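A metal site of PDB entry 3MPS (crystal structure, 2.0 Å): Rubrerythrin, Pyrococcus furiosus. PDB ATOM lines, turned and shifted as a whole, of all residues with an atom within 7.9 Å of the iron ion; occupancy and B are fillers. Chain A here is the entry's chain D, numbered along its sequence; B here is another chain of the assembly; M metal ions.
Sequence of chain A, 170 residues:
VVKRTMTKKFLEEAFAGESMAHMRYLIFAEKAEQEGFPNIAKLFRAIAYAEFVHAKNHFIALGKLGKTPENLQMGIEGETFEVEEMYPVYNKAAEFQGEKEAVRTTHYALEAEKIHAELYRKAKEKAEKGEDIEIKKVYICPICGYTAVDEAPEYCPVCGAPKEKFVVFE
N of Ala 161 lies close to SG of Cys 159 (3.6 Å).
N of Cys 156 is in hydrogen-bond range of O of Ala 161 (2.8 Å).
SG of Cys 156 lies close to N of Val 158 (3.6 Å).
SG of Cys 144 lies close to N of Tyr 146.
The backbone NH (N) of Ile 143 lies close to the side-chain sulfur (SG) of Cys 141, at 3.4 Å.
O of Tyr 146 sits at hydrogen-bond distance from N of Cys 141, at 2.9 Å.
Four residues have an atom within 4 Å of the iron ion: Cys 141, Cys 144, Cys 156 and Cys 159.
The nearest printed residue that does not touch the iron ion is Ile 143 (4.3 Å).
The side-chain sulfur (SG) of Cys 159 binds the iron ion.
SG of Cys 156 binds the iron ion (2.3 Å).
The iron ion is bound by SG of Cys 144.
SG of Cys 141 binds the iron ion, 2.3 Å away.
The iron ion has four donor atoms within binding distance.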
ATOM      1  N   TYR A 108      13.221  12.134  -1.776  1.00  0.00           N
ATOM      2  CA  TYR A 108      12.030  11.630  -2.513  1.00  0.00           C
ATOM      3  C   TYR A 108      11.373  12.727  -3.347  1.00  0.00           C
ATOM      4  O   TYR A 108      11.225  12.590  -4.576  1.00  0.00           O
ATOM      5  CB  TYR A 108      10.982  11.037  -1.552  1.00  0.00           C
ATOM      6  CG  TYR A 108      11.306   9.676  -0.992  1.00  0.00           C
ATOM      7  CD1 TYR A 108      12.283   8.868  -1.575  1.00  0.00           C
ATOM      8  CD2 TYR A 108      10.625   9.187   0.108  1.00  0.00           C
ATOM      9  CE1 TYR A 108      12.572   7.612  -1.058  1.00  0.00           C
ATOM     10  CE2 TYR A 108      10.897   7.914   0.627  1.00  0.00           C
ATOM     11  CZ  TYR A 108      11.885   7.145   0.031  1.00  0.00           C
ATOM     12  OH  TYR A 108      12.182   5.905   0.510  1.00  0.00           O
ATOM     13  N   ALA A 112      11.038  13.157  -7.323  1.00  0.00           N
ATOM     14  CA  ALA A 112       9.670  12.876  -7.759  1.00  0.00           C
ATOM     15  C   ALA A 112       8.930  14.116  -8.282  1.00  0.00           C
ATOM     16  O   ALA A 112       7.991  13.992  -9.067  1.00  0.00           O
ATOM     17  CB  ALA A 112       8.883  12.213  -6.627  1.00  0.00           C
ATOM     18  N   ILE A 140       0.758   7.220  -9.149  1.00  0.00           N
ATOM     19  CA  ILE A 140       1.542   7.871  -8.112  1.00  0.00           C
ATOM     20  C   ILE A 140       1.980   6.848  -7.081  1.00  0.00           C
ATOM     21  O   ILE A 140       1.177   6.047  -6.609  1.00  0.00           O
ATOM     22  CB  ILE A 140       0.794   9.046  -7.435  1.00  0.00           C
ATOM     23  CG1 ILE A 140       0.435  10.128  -8.470  1.00  0.00           C
ATOM     24  CG2 ILE A 140       1.654   9.719  -6.399  1.00  0.00           C
ATOM     25  CD1 ILE A 140      -0.920  10.025  -8.921  1.00  0.00           C
ATOM     26  N   CYS A 141       3.282   6.861  -6.781  1.00  0.00           N
ATOM     27  CA  CYS A 141       3.827   5.983  -5.776  1.00  0.00           C
ATOM     28  C   CYS A 141       3.458   6.484  -4.374  1.00  0.00           C
ATOM     29  O   CYS A 141       3.766   7.631  -4.031  1.00  0.00           O
ATOM     30  CB  CYS A 141       5.339   5.917  -5.916  1.00  0.00           C
ATOM     31  SG  CYS A 141       6.137   4.954  -4.610  1.00  0.00           S
ATOM     32  N   PRO A 142       2.810   5.623  -3.552  1.00  0.00           N
ATOM     33  CA  PRO A 142       2.367   6.004  -2.203  1.00  0.00           C
ATOM     34  C   PRO A 142       3.531   6.193  -1.206  1.00  0.00           C
ATOM     35  O   PRO A 142       3.304   6.741  -0.103  1.00  0.00           O
ATOM     36  CB  PRO A 142       1.499   4.819  -1.772  1.00  0.00           C
ATOM     37  CG  PRO A 142       2.075   3.651  -2.521  1.00  0.00           C
ATOM     38  CD  PRO A 142       2.464   4.227  -3.861  1.00  0.00           C
ATOM     39  N   ILE A 143       4.737   5.762  -1.575  1.00  0.00           N
ATOM     40  CA  ILE A 143       5.914   5.877  -0.711  1.00  0.00           C
ATOM     41  C   ILE A 143       6.644   7.226  -0.863  1.00  0.00           C
ATOM     42  O   ILE A 143       6.935   7.893   0.129  1.00  0.00           O
ATOM     43  CB  ILE A 143       6.914   4.720  -0.951  1.00  0.00           C
ATOM     44  CG1 ILE A 143       6.263   3.379  -0.636  1.00  0.00           C
ATOM     45  CG2 ILE A 143       8.171   4.880  -0.064  1.00  0.00           C
ATOM     46  CD1 ILE A 143       7.246   2.227  -0.518  1.00  0.00           C
ATOM     47  N   CYS A 144       6.900   7.611  -2.111  1.00  0.00           N
ATOM     48  CA  CYS A 144       7.804   8.705  -2.434  1.00  0.00           C
ATOM     49  C   CYS A 144       7.197   9.743  -3.371  1.00  0.00           C
ATOM     50  O   CYS A 144       7.840  10.755  -3.674  1.00  0.00           O
ATOM     51  CB  CYS A 144       9.068   8.128  -3.080  1.00  0.00           C
ATOM     52  SG  CYS A 144       8.819   7.517  -4.776  1.00  0.00           S
ATOM     53  N   GLY A 145       5.985   9.491  -3.852  1.00  0.00           N
ATOM     54  CA  GLY A 145       5.261  10.437  -4.711  1.00  0.00           C
ATOM     55  C   GLY A 145       5.651  10.414  -6.179  1.00  0.00           C
ATOM     56  O   GLY A 145       5.221  11.295  -6.958  1.00  0.00           O
ATOM     57  N   TYR A 146       6.443   9.417  -6.576  1.00  0.00           N
ATOM     58  CA  TYR A 146       6.887   9.285  -7.968  1.00  0.00           C
ATOM     59  C   TYR A 146       5.675   9.237  -8.898  1.00  0.00           C
ATOM     60  O   TYR A 146       4.734   8.470  -8.677  1.00  0.00           O
ATOM     61  CB  TYR A 146       7.813   8.076  -8.155  1.00  0.00           C
ATOM     62  CG  TYR A 146       8.506   8.038  -9.503  1.00  0.00           C
ATOM     63  CD1 TYR A 146       9.724   8.679  -9.699  1.00  0.00           C
ATOM     64  CD2 TYR A 146       7.959   7.344 -10.583  1.00  0.00           C
ATOM     65  CE1 TYR A 146      10.374   8.644 -10.918  1.00  0.00           C
ATOM     66  CE2 TYR A 146       8.595   7.315 -11.821  1.00  0.00           C
ATOM     67  CZ  TYR A 146       9.809   7.972 -11.973  1.00  0.00           C
ATOM     68  OH  TYR A 146      10.458   7.957 -13.181  1.00  0.00           O
ATOM     69  N   THR A 147       5.722  10.059  -9.929  1.00  0.00           N
ATOM     70  CA  THR A 147       4.565  10.336 -10.770  1.00  0.00           C
ATOM     71  C   THR A 147       4.865   9.906 -12.210  1.00  0.00           C
ATOM     72  O   THR A 147       5.864  10.328 -12.784  1.00  0.00           O
ATOM     73  CB  THR A 147       4.228  11.832 -10.728  1.00  0.00           C
ATOM     74  OG1 THR A 147       3.845  12.170  -9.383  1.00  0.00           O
ATOM     75  CG2 THR A 147       3.067  12.182 -11.700  1.00  0.00           C
ATOM     76  N   TYR A 155       9.422  -0.959 -11.568  1.00  0.00           N
ATOM     77  CA  TYR A 155       9.615  -0.568 -10.177  1.00  0.00           C
ATOM     78  C   TYR A 155       9.816   0.938 -10.088  1.00  0.00           C
ATOM     79  O   TYR A 155      10.190   1.580 -11.069  1.00  0.00           O
ATOM     80  CB  TYR A 155      10.783  -1.329  -9.525  1.00  0.00           C
ATOM     81  CG  TYR A 155      12.161  -0.957 -10.059  1.00  0.00           C
ATOM     82  CD1 TYR A 155      12.896   0.081  -9.480  1.00  0.00           C
ATOM     83  CD2 TYR A 155      12.737  -1.656 -11.118  1.00  0.00           C
ATOM     84  CE1 TYR A 155      14.150   0.431  -9.942  1.00  0.00           C
ATOM     85  CE2 TYR A 155      14.009  -1.314 -11.585  1.00  0.00           C
ATOM     86  CZ  TYR A 155      14.705  -0.273 -10.992  1.00  0.00           C
ATOM     87  OH  TYR A 155      15.950   0.080 -11.452  1.00  0.00           O
ATOM     88  N   CYS A 156       9.535   1.503  -8.917  1.00  0.00           N
ATOM     89  CA  CYS A 156       9.817   2.910  -8.656  1.00  0.00           C
ATOM     90  C   CYS A 156      11.332   3.163  -8.642  1.00  0.00           C
ATOM     91  O   CYS A 156      12.059   2.543  -7.853  1.00  0.00           O
ATOM     92  CB  CYS A 156       9.180   3.350  -7.338  1.00  0.00           C
ATOM     93  SG  CYS A 156       9.301   5.112  -7.012  1.00  0.00           S
ATOM     94  N   PRO A 157      11.817   4.065  -9.517  1.00  0.00           N
ATOM     95  CA  PRO A 157      13.238   4.408  -9.575  1.00  0.00           C
ATOM     96  C   PRO A 157      13.743   5.096  -8.303  1.00  0.00           C
ATOM     97  O   PRO A 157      14.934   5.066  -8.023  1.00  0.00           O
ATOM     98  CB  PRO A 157      13.341   5.380 -10.754  1.00  0.00           C
ATOM     99  CG  PRO A 157      12.059   5.182 -11.547  1.00  0.00           C
ATOM    100  CD  PRO A 157      11.038   4.806 -10.523  1.00  0.00           C
ATOM    101  N   VAL A 158      12.828   5.711  -7.565  1.00  0.00           N
ATOM    102  CA  VAL A 158      13.159   6.498  -6.393  1.00  0.00           C
ATOM    103  C   VAL A 158      13.176   5.627  -5.126  1.00  0.00           C
ATOM    104  O   VAL A 158      14.134   5.680  -4.370  1.00  0.00           O
ATOM    105  CB  VAL A 158      12.192   7.713  -6.247  1.00  0.00           C
ATOM    106  CG1 VAL A 158      12.510   8.520  -4.982  1.00  0.00           C
ATOM    107  CG2 VAL A 158      12.296   8.612  -7.478  1.00  0.00           C
ATOM    108  N   CYS A 159      12.136   4.852  -4.885  1.00  0.00           N
ATOM    109  CA  CYS A 159      12.047   4.087  -3.636  1.00  0.00           C
ATOM    110  C   CYS A 159      12.160   2.551  -3.752  1.00  0.00           C
ATOM    111  O   CYS A 159      12.284   1.877  -2.723  1.00  0.00           O
ATOM    112  CB  CYS A 159      10.786   4.476  -2.854  1.00  0.00           C
ATOM    113  SG  CYS A 159       9.196   3.734  -3.426  1.00  0.00           S
ATOM    114  N   GLY A 160      12.122   1.993  -4.966  1.00  0.00           N
ATOM    115  CA  GLY A 160      12.187   0.524  -5.157  1.00  0.00           C
ATOM    116  C   GLY A 160      10.866  -0.246  -5.202  1.00  0.00           C
ATOM    117  O   GLY A 160      10.810  -1.379  -5.706  1.00  0.00           O
ATOM    118  N   ALA A 161       9.795   0.378  -4.696  1.00  0.00           N
ATOM    119  CA  ALA A 161       8.443  -0.230  -4.730  1.00  0.00           C
ATOM    120  C   ALA A 161       8.056  -0.850  -6.083  1.00  0.00           C
ATOM    121  O   ALA A 161       8.260  -0.231  -7.130  1.00  0.00           O
ATOM    122  CB  ALA A 161       7.386   0.812  -4.312  1.00  0.00           C
ATOM    123  N   PRO A 162       7.522  -2.091  -6.071  1.00  0.00           N
ATOM    124  CA  PRO A 162       7.021  -2.718  -7.298  1.00  0.00           C
ATOM    125  C   PRO A 162       5.901  -1.939  -8.009  1.00  0.00           C
ATOM    126  O   PRO A 162       5.168  -1.166  -7.373  1.00  0.00           O
ATOM    127  CB  PRO A 162       6.507  -4.089  -6.833  1.00  0.00           C
ATOM    128  CG  PRO A 162       6.383  -3.994  -5.345  1.00  0.00           C
ATOM    129  CD  PRO A 162       7.395  -2.981  -4.903  1.00  0.00           C
ATOM    130  N   LYS A 165       2.316  -1.398  -6.453  1.00  0.00           N
ATOM    131  CA  LYS A 165       2.055  -0.566  -5.283  1.00  0.00           C
ATOM    132  C   LYS A 165       1.535   0.822  -5.696  1.00  0.00           C
ATOM    133  O   LYS A 165       0.906   1.501  -4.897  1.00  0.00           O
ATOM    134  CB  LYS A 165       3.307  -0.423  -4.429  1.00  0.00           C
ATOM    135  CG  LYS A 165       3.885  -1.767  -3.947  1.00  0.00           C
ATOM    136  CD  LYS A 165       3.339  -2.168  -2.585  1.00  0.00           C
ATOM    137  CE  LYS A 165       3.721  -3.597  -2.213  1.00  0.00           C
ATOM    138  NZ  LYS A 165       2.883  -4.591  -2.959  1.00  0.00           N
ATOM    139  N   PHE A 166       1.792   1.206  -6.944  1.00  0.00           N
ATOM    140  CA  PHE A 166       1.408   2.520  -7.449  1.00  0.00           C
ATOM    141  C   PHE A 166      -0.110   2.727  -7.378  1.00  0.00           C
ATOM    142  O   PHE A 166      -0.886   1.822  -7.721  1.00  0.00           O
ATOM    143  CB  PHE A 166       1.891   2.685  -8.894  1.00  0.00           C
ATOM    144  CG  PHE A 166       3.336   3.120  -9.006  1.00  0.00           C
ATOM    145  CD1 PHE A 166       3.657   4.425  -9.342  1.00  0.00           C
ATOM    146  CD2 PHE A 166       4.372   2.207  -8.802  1.00  0.00           C
ATOM    147  CE1 PHE A 166       5.004   4.836  -9.452  1.00  0.00           C
ATOM    148  CE2 PHE A 166       5.714   2.610  -8.916  1.00  0.00           C
ATOM    149  CZ  PHE A 166       6.026   3.919  -9.250  1.00  0.00           C
ATOM    150  N   VAL B  53       1.512  12.753  -0.237  1.00  0.00           N
ATOM    151  CA  VAL B  53       2.608  11.855   0.134  1.00  0.00           C
ATOM    152  C   VAL B  53       3.807  12.630   0.689  1.00  0.00           C
ATOM    153  O   VAL B  53       4.343  12.277   1.736  1.00  0.00           O
ATOM    154  CB  VAL B  53       3.033  10.933  -1.034  1.00  0.00           C
ATOM    155  CG1 VAL B  53       4.224  10.022  -0.617  1.00  0.00           C
ATOM    156  CG2 VAL B  53       1.847  10.072  -1.489  1.00  0.00           C
HETATM  157 FE    FE M   1       8.392   5.267  -4.917  1.00  0.00          FE
